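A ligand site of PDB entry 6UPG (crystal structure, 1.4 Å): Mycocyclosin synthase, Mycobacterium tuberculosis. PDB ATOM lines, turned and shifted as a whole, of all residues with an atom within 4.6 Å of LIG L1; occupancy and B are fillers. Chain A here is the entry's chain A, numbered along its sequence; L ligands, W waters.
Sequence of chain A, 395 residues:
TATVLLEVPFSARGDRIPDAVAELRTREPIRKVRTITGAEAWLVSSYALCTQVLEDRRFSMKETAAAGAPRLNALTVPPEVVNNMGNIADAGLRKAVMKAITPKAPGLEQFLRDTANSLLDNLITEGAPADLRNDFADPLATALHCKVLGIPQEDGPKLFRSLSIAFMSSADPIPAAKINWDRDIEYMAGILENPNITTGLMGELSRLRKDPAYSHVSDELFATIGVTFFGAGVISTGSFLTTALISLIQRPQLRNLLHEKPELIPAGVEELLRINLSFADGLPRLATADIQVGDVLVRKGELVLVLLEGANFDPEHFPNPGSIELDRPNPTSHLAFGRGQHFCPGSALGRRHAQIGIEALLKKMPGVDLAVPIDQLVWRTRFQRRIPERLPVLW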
ATOM      1  N   MET A  61      25.244  22.011 -13.198  1.00  0.00           N
ATOM      2  CA  MET A  61      25.625  22.249 -11.813  1.00  0.00           C
ATOM      3  C   MET A  61      26.874  21.441 -11.453  1.00  0.00           C
ATOM      4  O   MET A  61      27.829  21.965 -10.866  1.00  0.00           O
ATOM      5  CB  MET A  61      24.467  21.910 -10.869  1.00  0.00           C
ATOM      6  CG  MET A  61      24.872  21.800  -9.388  1.00  0.00           C
ATOM      7  SD  MET A  61      23.468  21.232  -8.375  1.00  0.00           S
ATOM      8  CE  MET A  61      22.406  22.646  -8.535  1.00  0.00           C
ATOM      9  N   MET A  85      22.373  15.614  -5.507  1.00  0.00           N
ATOM     10  CA  MET A  85      21.103  15.018  -5.899  1.00  0.00           C
ATOM     11  C   MET A  85      21.297  13.986  -6.996  1.00  0.00           C
ATOM     12  O   MET A  85      20.608  12.958  -7.015  1.00  0.00           O
ATOM     13  CB  MET A  85      20.101  16.093  -6.323  1.00  0.00           C
ATOM     14  CG  MET A  85      18.795  15.516  -6.821  1.00  0.00           C
ATOM     15  SD  MET A  85      18.057  14.367  -5.665  1.00  0.00           S
ATOM     16  CE  MET A  85      18.070  15.432  -4.260  1.00  0.00           C
ATOM     17  N   ARG A  94      16.347   8.440  -4.669  1.00  0.00           N
ATOM     18  CA  ARG A  94      15.622   9.702  -4.837  1.00  0.00           C
ATOM     19  C   ARG A  94      14.196   9.604  -4.297  1.00  0.00           C
ATOM     20  O   ARG A  94      13.753  10.478  -3.541  1.00  0.00           O
ATOM     21  CB  ARG A  94      15.620  10.152  -6.291  1.00  0.00           C
ATOM     22  CG  ARG A  94      14.932  11.506  -6.507  1.00  0.00           C
ATOM     23  CD  ARG A  94      14.913  11.906  -7.979  1.00  0.00           C
ATOM     24  NE  ARG A  94      14.738  13.340  -8.115  1.00  0.00           N
ATOM     25  CZ  ARG A  94      15.723  14.197  -8.407  1.00  0.00           C
ATOM     26  NH1 ARG A  94      16.954  13.734  -8.635  1.00  0.00           N
ATOM     27  NH2 ARG A  94      15.479  15.495  -8.494  1.00  0.00           N
ATOM     28  N   ILE A 101      10.804  13.763   3.104  1.00  0.00           N
ATOM     29  CA  ILE A 101      10.895  15.191   3.355  1.00  0.00           C
ATOM     30  C   ILE A 101       9.632  15.942   2.928  1.00  0.00           C
ATOM     31  O   ILE A 101       9.650  17.172   2.837  1.00  0.00           O
ATOM     32  CB  ILE A 101      12.163  15.823   2.764  1.00  0.00           C
ATOM     33  CG1 ILE A 101      12.129  15.798   1.238  1.00  0.00           C
ATOM     34  CG2 ILE A 101      13.401  15.115   3.309  1.00  0.00           C
ATOM     35  CD1 ILE A 101      13.260  16.559   0.586  1.00  0.00           C
ATOM     36  N   HIS A 145      13.744  20.095  11.023  1.00  0.00           N
ATOM     37  CA  HIS A 145      14.627  19.207  10.304  1.00  0.00           C
ATOM     38  C   HIS A 145      15.139  18.067  11.169  1.00  0.00           C
ATOM     39  O   HIS A 145      15.385  16.982  10.647  1.00  0.00           O
ATOM     40  CB  HIS A 145      15.752  19.976   9.612  1.00  0.00           C
ATOM     41  CG  HIS A 145      15.272  20.684   8.392  1.00  0.00           C
ATOM     42  ND1 HIS A 145      14.561  21.851   8.450  1.00  0.00           N
ATOM     43  CD2 HIS A 145      15.321  20.335   7.081  1.00  0.00           C
ATOM     44  CE1 HIS A 145      14.205  22.217   7.219  1.00  0.00           C
ATOM     45  NE2 HIS A 145      14.655  21.308   6.377  1.00  0.00           N
ATOM     46  N   PHE A 229      20.978  17.466   3.682  1.00  0.00           N
ATOM     47  CA  PHE A 229      19.570  17.813   3.761  1.00  0.00           C
ATOM     48  C   PHE A 229      19.270  18.618   5.012  1.00  0.00           C
ATOM     49  O   PHE A 229      18.462  19.554   4.970  1.00  0.00           O
ATOM     50  CB  PHE A 229      18.678  16.574   3.591  1.00  0.00           C
ATOM     51  CG  PHE A 229      18.413  16.256   2.146  1.00  0.00           C
ATOM     52  CD1 PHE A 229      19.464  15.864   1.321  1.00  0.00           C
ATOM     53  CD2 PHE A 229      17.152  16.419   1.586  1.00  0.00           C
ATOM     54  CE1 PHE A 229      19.257  15.608  -0.021  1.00  0.00           C
ATOM     55  CE2 PHE A 229      16.947  16.159   0.231  1.00  0.00           C
ATOM     56  CZ  PHE A 229      17.993  15.757  -0.564  1.00  0.00           C
ATOM     57  N   ALA A 232      21.027  22.307   3.924  1.00  0.00           N
ATOM     58  CA  ALA A 232      20.285  23.028   2.900  1.00  0.00           C
ATOM     59  C   ALA A 232      18.878  23.345   3.363  1.00  0.00           C
ATOM     60  O   ALA A 232      18.378  24.462   3.154  1.00  0.00           O
ATOM     61  CB  ALA A 232      20.250  22.216   1.595  1.00  0.00           C
ATOM     62  N   GLY A 233      18.216  22.386   4.015  1.00  0.00           N
ATOM     63  CA  GLY A 233      16.849  22.634   4.458  1.00  0.00           C
ATOM     64  C   GLY A 233      16.781  23.690   5.551  1.00  0.00           C
ATOM     65  O   GLY A 233      15.945  24.594   5.491  1.00  0.00           O
ATOM     66  N   SER A 236      17.777  27.204   4.298  1.00  0.00           N
ATOM     67  CA  SER A 236      16.869  27.757   3.302  1.00  0.00           C
ATOM     68  C   SER A 236      15.538  28.125   3.925  1.00  0.00           C
ATOM     69  O   SER A 236      15.023  29.228   3.680  1.00  0.00           O
ATOM     70  CB  SER A 236      16.685  26.750   2.167  1.00  0.00           C
ATOM     71  OG  SER A 236      17.932  26.521   1.518  1.00  0.00           O
ATOM     72  N   THR A 237      14.984  27.244   4.764  1.00  0.00           N
ATOM     73  CA  THR A 237      13.724  27.554   5.419  1.00  0.00           C
ATOM     74  C   THR A 237      13.901  28.648   6.471  1.00  0.00           C
ATOM     75  O   THR A 237      13.065  29.556   6.571  1.00  0.00           O
ATOM     76  CB  THR A 237      13.095  26.307   6.056  1.00  0.00           C
ATOM     77  OG1 THR A 237      13.975  25.723   7.034  1.00  0.00           O
ATOM     78  CG2 THR A 237      12.741  25.274   4.993  1.00  0.00           C
ATOM     79  N   PHE A 240      14.497  31.974   4.554  1.00  0.00           N
ATOM     80  CA  PHE A 240      13.306  32.444   3.863  1.00  0.00           C
ATOM     81  C   PHE A 240      12.269  32.953   4.852  1.00  0.00           C
ATOM     82  O   PHE A 240      11.697  34.036   4.672  1.00  0.00           O
ATOM     83  CB  PHE A 240      12.677  31.369   2.987  1.00  0.00           C
ATOM     84  CG  PHE A 240      11.316  31.776   2.510  1.00  0.00           C
ATOM     85  CD1 PHE A 240      11.183  32.890   1.705  1.00  0.00           C
ATOM     86  CD2 PHE A 240      10.168  31.117   2.964  1.00  0.00           C
ATOM     87  CE1 PHE A 240       9.928  33.337   1.307  1.00  0.00           C
ATOM     88  CE2 PHE A 240       8.918  31.557   2.561  1.00  0.00           C
ATOM     89  CZ  PHE A 240       8.799  32.665   1.737  1.00  0.00           C
ATOM     90  N   LEU A 273       7.398  34.120  -1.285  1.00  0.00           N
ATOM     91  CA  LEU A 273       8.432  33.369  -1.997  1.00  0.00           C
ATOM     92  C   LEU A 273       8.846  34.083  -3.269  1.00  0.00           C
ATOM     93  O   LEU A 273      10.039  34.266  -3.532  1.00  0.00           O
ATOM     94  CB  LEU A 273       7.919  31.962  -2.320  1.00  0.00           C
ATOM     95  CG  LEU A 273       7.934  30.977  -1.159  1.00  0.00           C
ATOM     96  CD1 LEU A 273       6.999  29.807  -1.457  1.00  0.00           C
ATOM     97  CD2 LEU A 273       9.359  30.476  -0.915  1.00  0.00           C
ATOM     98  N   PHE A 279      18.261  34.244  -1.553  1.00  0.00           N
ATOM     99  CA  PHE A 279      19.462  33.780  -2.250  1.00  0.00           C
ATOM    100  C   PHE A 279      20.357  34.961  -2.573  1.00  0.00           C
ATOM    101  O   PHE A 279      19.981  35.860  -3.327  1.00  0.00           O
ATOM    102  CB  PHE A 279      19.116  32.963  -3.501  1.00  0.00           C
ATOM    103  CG  PHE A 279      18.887  31.506  -3.225  1.00  0.00           C
ATOM    104  CD1 PHE A 279      17.805  31.094  -2.473  1.00  0.00           C
ATOM    105  CD2 PHE A 279      19.778  30.534  -3.678  1.00  0.00           C
ATOM    106  CE1 PHE A 279      17.595  29.742  -2.200  1.00  0.00           C
ATOM    107  CE2 PHE A 279      19.575  29.190  -3.391  1.00  0.00           C
ATOM    108  CZ  PHE A 279      18.483  28.794  -2.652  1.00  0.00           C
ATOM    109  N   LEU A 283      22.227  31.478  -9.098  1.00  0.00           N
ATOM    110  CA  LEU A 283      22.481  30.044  -9.122  1.00  0.00           C
ATOM    111  C   LEU A 283      23.553  29.746 -10.161  1.00  0.00           C
ATOM    112  O   LEU A 283      23.410  30.147 -11.312  1.00  0.00           O
ATOM    113  CB  LEU A 283      21.212  29.272  -9.504  1.00  0.00           C
ATOM    114  CG  LEU A 283      20.011  29.471  -8.575  1.00  0.00           C
ATOM    115  CD1 LEU A 283      18.894  28.558  -9.055  1.00  0.00           C
ATOM    116  CD2 LEU A 283      20.374  29.196  -7.124  1.00  0.00           C
ATOM    117  N   ARG A 285      26.012  27.792 -12.872  1.00  0.00           N
ATOM    118  CA  ARG A 285      26.040  26.708 -13.853  1.00  0.00           C
ATOM    119  C   ARG A 285      27.275  26.903 -14.726  1.00  0.00           C
ATOM    120  O   ARG A 285      27.662  28.038 -15.013  1.00  0.00           O
ATOM    121  CB  ARG A 285      24.802  26.726 -14.770  1.00  0.00           C
ATOM    122  CG  ARG A 285      23.462  26.490 -14.079  1.00  0.00           C
ATOM    123  CD  ARG A 285      23.349  25.081 -13.519  1.00  0.00           C
ATOM    124  NE  ARG A 285      21.986  24.779 -13.079  1.00  0.00           N
ATOM    125  CZ  ARG A 285      21.523  24.961 -11.849  1.00  0.00           C
ATOM    126  NH1 ARG A 285      22.303  25.455 -10.895  1.00  0.00           N
ATOM    127  NH2 ARG A 285      20.270  24.647 -11.560  1.00  0.00           N
ATOM    128  N   LEU A 308      17.860  34.916  -9.363  1.00  0.00           N
ATOM    129  CA  LEU A 308      16.466  34.544  -9.094  1.00  0.00           C
ATOM    130  C   LEU A 308      15.572  35.783  -9.006  1.00  0.00           C
ATOM    131  O   LEU A 308      14.442  35.767  -9.516  1.00  0.00           O
ATOM    132  CB  LEU A 308      16.366  33.695  -7.837  1.00  0.00           C
ATOM    133  CG  LEU A 308      17.067  32.333  -7.890  1.00  0.00           C
ATOM    134  CD1 LEU A 308      16.832  31.534  -6.629  1.00  0.00           C
ATOM    135  CD2 LEU A 308      16.611  31.543  -9.120  1.00  0.00           C
ATOM    136  N   LEU A 335      10.672  31.454  -9.618  1.00  0.00           N
ATOM    137  CA  LEU A 335      11.851  30.599  -9.567  1.00  0.00           C
ATOM    138  C   LEU A 335      12.451  30.493  -8.163  1.00  0.00           C
ATOM    139  O   LEU A 335      13.615  30.132  -8.030  1.00  0.00           O
ATOM    140  CB  LEU A 335      12.901  31.078 -10.563  1.00  0.00           C
ATOM    141  CG  LEU A 335      12.473  31.305 -12.018  1.00  0.00           C
ATOM    142  CD1 LEU A 335      13.696  31.477 -12.908  1.00  0.00           C
ATOM    143  CD2 LEU A 335      11.594  30.171 -12.531  1.00  0.00           C
ATOM    144  N   ALA A 336      11.653  30.762  -7.115  1.00  0.00           N
ATOM    145  CA  ALA A 336      12.192  30.716  -5.757  1.00  0.00           C
ATOM    146  C   ALA A 336      12.722  29.340  -5.380  1.00  0.00           C
ATOM    147  O   ALA A 336      13.635  29.240  -4.554  1.00  0.00           O
ATOM    148  CB  ALA A 336      11.148  31.162  -4.738  1.00  0.00           C
ATOM    149  N   PHE A 337      12.182  28.281  -5.968  1.00  0.00           N
ATOM    150  CA  PHE A 337      12.645  26.913  -5.751  1.00  0.00           C
ATOM    151  C   PHE A 337      13.454  26.389  -6.930  1.00  0.00           C
ATOM    152  O   PHE A 337      13.635  25.171  -7.050  1.00  0.00           O
ATOM    153  CB  PHE A 337      11.456  25.986  -5.476  1.00  0.00           C
ATOM    154  CG  PHE A 337      10.728  26.262  -4.183  1.00  0.00           C
ATOM    155  CD1 PHE A 337      11.375  26.092  -2.970  1.00  0.00           C
ATOM    156  CD2 PHE A 337       9.393  26.640  -4.191  1.00  0.00           C
ATOM    157  CE1 PHE A 337      10.708  26.340  -1.765  1.00  0.00           C
ATOM    158  CE2 PHE A 337       8.724  26.892  -2.994  1.00  0.00           C
ATOM    159  CZ  PHE A 337       9.376  26.732  -1.790  1.00  0.00           C
ATOM    160  N   GLY A 338      13.902  27.270  -7.806  1.00  0.00           N
ATOM    161  CA  GLY A 338      14.588  26.834  -9.012  1.00  0.00           C
ATOM    162  C   GLY A 338      13.618  26.361 -10.072  1.00  0.00           C
ATOM    163  O   GLY A 338      12.421  26.665 -10.063  1.00  0.00           O
ATOM    164  N   GLN A 341      16.043  20.434 -13.827  1.00  0.00           N
ATOM    165  CA  GLN A 341      16.641  19.241 -13.238  1.00  0.00           C
ATOM    166  C   GLN A 341      16.853  19.395 -11.728  1.00  0.00           C
ATOM    167  O   GLN A 341      16.688  18.427 -10.974  1.00  0.00           O
ATOM    168  CB  GLN A 341      17.965  18.940 -13.931  1.00  0.00           C
ATOM    169  CG  GLN A 341      18.725  17.747 -13.378  1.00  0.00           C
ATOM    170  CD  GLN A 341      18.123  16.427 -13.817  1.00  0.00           C
ATOM    171  OE1 GLN A 341      17.225  16.384 -14.656  1.00  0.00           O
ATOM    172  NE2 GLN A 341      18.625  15.334 -13.246  1.00  0.00           N
ATOM    173  N   HIS A 342      17.215  20.591 -11.275  1.00  0.00           N
ATOM    174  CA  HIS A 342      17.601  20.801  -9.881  1.00  0.00           C
ATOM    175  C   HIS A 342      16.512  21.452  -9.040  1.00  0.00           C
ATOM    176  O   HIS A 342      16.814  21.989  -7.972  1.00  0.00           O
ATOM    177  CB  HIS A 342      18.904  21.586  -9.822  1.00  0.00           C
ATOM    178  CG  HIS A 342      20.055  20.876 -10.447  1.00  0.00           C
ATOM    179  ND1 HIS A 342      20.741  19.869  -9.798  1.00  0.00           N
ATOM    180  CD2 HIS A 342      20.608  20.972 -11.678  1.00  0.00           C
ATOM    181  CE1 HIS A 342      21.679  19.392 -10.595  1.00  0.00           C
ATOM    182  NE2 HIS A 342      21.628  20.048 -11.748  1.00  0.00           N
ATOM    183  N   PHE A 343      15.257  21.394  -9.497  1.00  0.00           N
ATOM    184  CA  PHE A 343      14.158  21.981  -8.751  1.00  0.00           C
ATOM    185  C   PHE A 343      14.148  21.435  -7.326  1.00  0.00           C
ATOM    186  O   PHE A 343      14.333  20.238  -7.096  1.00  0.00           O
ATOM    187  CB  PHE A 343      12.833  21.644  -9.441  1.00  0.00           C
ATOM    188  CG  PHE A 343      11.643  22.225  -8.750  1.00  0.00           C
ATOM    189  CD1 PHE A 343      11.258  23.521  -8.990  1.00  0.00           C
ATOM    190  CD2 PHE A 343      10.919  21.474  -7.837  1.00  0.00           C
ATOM    191  CE1 PHE A 343      10.158  24.089  -8.342  1.00  0.00           C
ATOM    192  CE2 PHE A 343       9.824  22.034  -7.172  1.00  0.00           C
ATOM    193  CZ  PHE A 343       9.455  23.341  -7.434  1.00  0.00           C
ATOM    194  N   CYS A 344      13.948  22.338  -6.366  1.00  0.00           N
ATOM    195  CA  CYS A 344      14.078  22.002  -4.954  1.00  0.00           C
ATOM    196  C   CYS A 344      13.235  20.794  -4.579  1.00  0.00           C
ATOM    197  O   CYS A 344      12.004  20.819  -4.767  1.00  0.00           O
ATOM    198  CB  CYS A 344      13.621  23.194  -4.128  1.00  0.00           C
ATOM    199  SG  CYS A 344      13.652  22.859  -2.369  1.00  0.00           S
ATOM    200  N   PRO A 345      13.830  19.741  -4.005  1.00  0.00           N
ATOM    201  CA  PRO A 345      13.039  18.582  -3.576  1.00  0.00           C
ATOM    202  C   PRO A 345      12.302  18.816  -2.266  1.00  0.00           C
ATOM    203  O   PRO A 345      11.488  17.968  -1.871  1.00  0.00           O
ATOM    204  CB  PRO A 345      14.102  17.477  -3.424  1.00  0.00           C
ATOM    205  CG  PRO A 345      15.346  18.253  -2.987  1.00  0.00           C
ATOM    206  CD  PRO A 345      15.273  19.559  -3.768  1.00  0.00           C
ATOM    207  N   GLY A 346      12.577  19.931  -1.598  1.00  0.00           N
ATOM    208  CA  GLY A 346      11.915  20.211  -0.333  1.00  0.00           C
ATOM    209  C   GLY A 346      10.902  21.334  -0.424  1.00  0.00           C
ATOM    210  O   GLY A 346      10.554  21.921   0.605  1.00  0.00           O
ATOM    211  N   LEU A 349       7.801  21.139   1.889  1.00  0.00           N
ATOM    212  CA  LEU A 349       8.160  21.317   3.288  1.00  0.00           C
ATOM    213  C   LEU A 349       8.514  22.776   3.567  1.00  0.00           C
ATOM    214  O   LEU A 349       8.151  23.312   4.623  1.00  0.00           O
ATOM    215  CB  LEU A 349       9.330  20.409   3.647  1.00  0.00           C
ATOM    216  CG  LEU A 349       9.743  20.324   5.115  1.00  0.00           C
ATOM    217  CD1 LEU A 349       8.618  19.753   5.976  1.00  0.00           C
ATOM    218  CD2 LEU A 349      11.012  19.498   5.289  1.00  0.00           C
ATOM    219  N   GLY A 350       9.214  23.430   2.639  1.00  0.00           N
ATOM    220  CA  GLY A 350       9.532  24.829   2.833  1.00  0.00           C
ATOM    221  C   GLY A 350       8.296  25.704   2.865  1.00  0.00           C
ATOM    222  O   GLY A 350       8.186  26.608   3.697  1.00  0.00           O
HETATM  223  C1  LIG L   1      17.575  23.032  -4.442  1.00  0.00           C
HETATM  224  C2  LIG L   1      15.437  26.989  -2.683  1.00  0.00           C
HETATM  225  C3  LIG L   1      13.953  24.395   1.123  1.00  0.00           C
HETATM  226  C4  LIG L   1      16.975  20.824  -0.170  1.00  0.00           C
HETATM  227  C5  LIG L   1      17.066  24.309  -4.347  1.00  0.00           C
HETATM  228  C6  LIG L   1      17.154  25.339  -5.357  1.00  0.00           C
HETATM  229  C7  LIG L   1      16.553  26.432  -4.866  1.00  0.00           C
HETATM  230  C8  LIG L   1      16.086  26.138  -3.534  1.00  0.00           C
HETATM  231  C9  LIG L   1      16.403  27.808  -5.558  1.00  0.00           C
HETATM  232  C10 LIG L   1      17.797  25.163  -6.762  1.00  0.00           C
HETATM  233  C11 LIG L   1      19.311  25.286  -6.691  1.00  0.00           C
HETATM  234  C12 LIG L   1      19.914  25.256  -8.074  1.00  0.00           C
HETATM  235  O1  LIG L   1      21.134  25.533  -8.188  1.00  0.00           O
HETATM  236  O2  LIG L   1      19.198  24.963  -9.057  1.00  0.00           O
HETATM  237  C13 LIG L   1      14.824  26.623  -1.501  1.00  0.00           C
HETATM  238  C14 LIG L   1      13.972  27.481  -0.702  1.00  0.00           C
HETATM  239  C15 LIG L   1      13.568  26.764   0.373  1.00  0.00           C
HETATM  240  C16 LIG L   1      14.141  25.438   0.248  1.00  0.00           C
HETATM  241  C17 LIG L   1      13.646  28.947  -1.052  1.00  0.00           C
HETATM  242  C18 LIG L   1      12.636  27.163   1.531  1.00  0.00           C
HETATM  243  C19 LIG L   1      11.719  28.124   1.452  1.00  0.00           C
HETATM  244  C20 LIG L   1      14.613  23.179   1.092  1.00  0.00           C
HETATM  245  C21 LIG L   1      14.430  22.090   2.023  1.00  0.00           C
HETATM  246  C22 LIG L   1      15.272  21.106   1.670  1.00  0.00           C
HETATM  247  C23 LIG L   1      16.003  21.547   0.499  1.00  0.00           C
HETATM  248  C24 LIG L   1      13.429  22.118   3.203  1.00  0.00           C
HETATM  249  C25 LIG L   1      15.508  19.720   2.310  1.00  0.00           C
HETATM  250  C26 LIG L   1      14.994  19.305   3.475  1.00  0.00           C
HETATM  251  C27 LIG L   1      17.422  21.114  -1.430  1.00  0.00           C
HETATM  252  C28 LIG L   1      18.344  20.315  -2.233  1.00  0.00           C
HETATM  253  C29 LIG L   1      18.506  20.926  -3.411  1.00  0.00           C
HETATM  254  C30 LIG L   1      17.700  22.133  -3.399  1.00  0.00           C
HETATM  255  C31 LIG L   1      19.000  19.001  -1.774  1.00  0.00           C
HETATM  256  C32 LIG L   1      19.379  20.431  -4.597  1.00  0.00           C
HETATM  257  C33 LIG L   1      18.468  19.725  -5.610  1.00  0.00           C
HETATM  258  C34 LIG L   1      19.187  19.290  -6.870  1.00  0.00           C
HETATM  259  O3  LIG L   1      20.378  19.652  -7.062  1.00  0.00           O
HETATM  260  O4  LIG L   1      18.557  18.589  -7.690  1.00  0.00           O
HETATM  261  N1  LIG L   1      16.401  24.824  -3.248  1.00  0.00           N
HETATM  262  N2  LIG L   1      14.916  25.398  -0.893  1.00  0.00           N
HETATM  263  N3  LIG L   1      15.566  22.810   0.158  1.00  0.00           N
HETATM  264  N4  LIG L   1      17.059  22.224  -2.170  1.00  0.00           N
HETATM  265 FE1  LIG L   1      15.784  23.719  -1.629  1.00  0.00          FE
HETATM  266  C1  LG2 L   2      23.520  19.871  -2.337  1.00  0.00           C
HETATM  267  C2  LG2 L   2      25.811  21.373  -3.249  1.00  0.00           C
HETATM  268  N1  LG2 L   2      23.710  20.137  -3.738  1.00  0.00           N
HETATM  269  O1  LG2 L   2      26.819  21.898  -3.620  1.00  0.00           O
HETATM  270  C3  LG2 L   2      24.482  21.180   1.882  1.00  0.00           C
HETATM  271  C4  LG2 L   2      25.655  22.824   0.599  1.00  0.00           C
HETATM  272  C5  LG2 L   2      21.930  22.746  -3.973  1.00  0.00           C
HETATM  273  C6  LG2 L   2      25.328  21.412   2.959  1.00  0.00           C
HETATM  274  C7  LG2 L   2      26.499  23.061   1.667  1.00  0.00           C
HETATM  275  C8  LG2 L   2      21.011  23.543  -3.057  1.00  0.00           C
HETATM  276  C9  LG2 L   2      24.448  20.471  -1.286  1.00  0.00           C
HETATM  277  C10 LG2 L   2      24.752  20.991  -4.287  1.00  0.00           C
HETATM  278  C11 LG2 L   2      19.319  25.058  -1.657  1.00  0.00           C
HETATM  279  C12 LG2 L   2      23.711  21.564  -0.482  1.00  0.00           C
HETATM  280  C13 LG2 L   2      24.144  22.238  -4.951  1.00  0.00           C
HETATM  281  C14 LG2 L   2      23.783  24.150  -3.164  1.00  0.00           C
HETATM  282  C15 LG2 L   2      22.989  24.834  -2.371  1.00  0.00           C
HETATM  283  C16 LG2 L   2      24.641  21.873   0.697  1.00  0.00           C
HETATM  284  C17 LG2 L   2      23.219  23.026  -4.026  1.00  0.00           C
HETATM  285  C18 LG2 L   2      26.351  22.348   2.851  1.00  0.00           C
HETATM  286  C19 LG2 L   2      21.515  24.511  -2.318  1.00  0.00           C
HETATM  287  N2  LG2 L   2      25.636  21.080  -1.854  1.00  0.00           N
HETATM  288  O2  LG2 L   2      22.637  19.155  -1.987  1.00  0.00           O
HETATM  289  O3  LG2 L   2      27.211  22.557   3.936  1.00  0.00           O
HETATM  290  O4  LG2 L   2      20.703  25.265  -1.464  1.00  0.00           O
HETATM  291  O   HOH W   1      15.904  17.927  -7.301  1.00  0.00           O
HETATM  292  O   HOH W   2      22.660  25.926  -5.973  1.00  0.00           O
HETATM  293  O   HOH W   3      19.233  16.826  -9.670  1.00  0.00           O
HETATM  294  O   HOH W   4      22.528  18.573  -5.826  1.00  0.00           O
HETATM  295  O   HOH W   5      16.789  24.690 -10.234  1.00  0.00           O
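NH2 of Arg 285 lies within salt-bridge range of O2 of LIG L1, 2.7 Å away. A ring nitrogen (ND1) of His 342 is in hydrogen-bond range of an oxygen (O3) of LIG L1, 2.8 Å away. The side-chain sulfur of Cys 344 is bound to an iron atom (FE1) of LIG L1.
The backbone carbonyl oxygen (O) of Gly 233 lies within hydrogen-bond range of the side-chain hydroxyl (OG1) of Thr 237 (2.7 Å). SD of Met 85 sits close to NH1 of Arg 94. N of Gly 346 sits close to SG of Cys 344, at 3.2 Å. N of Cys 344 is in hydrogen-bond range of O of Phe 337, 2.9 Å away. The side-chain hydroxyl (OG) of Ser 236 sits at hydrogen-bond distance from the backbone carbonyl oxygen (O) of Ala 232. ND1 of His 342 sits at hydrogen-bond distance from SD of Met 61 (3.4 Å).
An oxygen (O3) of LIG L1 sits close to the side-chain sulfur (SD) of Met 61 (3.7 Å). Met 85 touches LIG L1. His 145 touches LIG L1. Phe 229 touches LIG L1. Ala 232 touches LIG L1. Gly 233 touches LIG L1 (CA to C21, 3.5 Å). Ser 236 touches LIG L1 (CB to C16, 3.4 Å). Thr 237 touches LIG L1 (CG2 to C24, 3.7 Å). CD2 of Phe 240 touches C19 of LIG L1, 3.7 Å away. CE1 of Phe 279 touches C2 of LIG L1 (3.5 Å). Leu 283 touches LIG L1 (CD1 to C12, 3.6 Å). CD1 of Leu 308 touches C9 of LIG L1 (3.9 Å). O of Ala 336 touches C9 of LIG L1, at 3.3 Å. Phe 337 touches LIG L1. N of Gly 338 touches C9 of LIG L1 (3.4 Å). O of Gln 341 touches O4 of LIG L1 (3.8 Å). Pro 345 touches LIG L1. O of Gly 346 touches C24 of LIG L1 (3.9 Å). 21 residues have an atom within 4 Å of LIG L1: Met 61, Met 85, His 145, Phe 229, Ala 232, Gly 233, Ser 236, Thr 237, Phe 240, Phe 279, Leu 283, Arg 285, Leu 308, Ala 336, Phe 337, Gly 338, Gln 341, His 342, Cys 344, Pro 345 and Gly 346. The nearest printed residue that does not touch LIG L1 is Leu 273 (4.1 Å).
Water W4 lies within hydrogen-bond range of an oxygen (O3) of LIG L1, a nitrogen (N1) of LG2 L2 and the backbone NH (N) of Met 85. Water W3 lies within hydrogen-bond range of O4 of LIG L1, O of Gln 341 and ND1 of His 342. Water W1 lies within hydrogen-bond range of the guanidinium group (NH2) of Arg 94, an oxygen (O4) of LIG L1 and the backbone carbonyl oxygen (O) of Phe 343.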
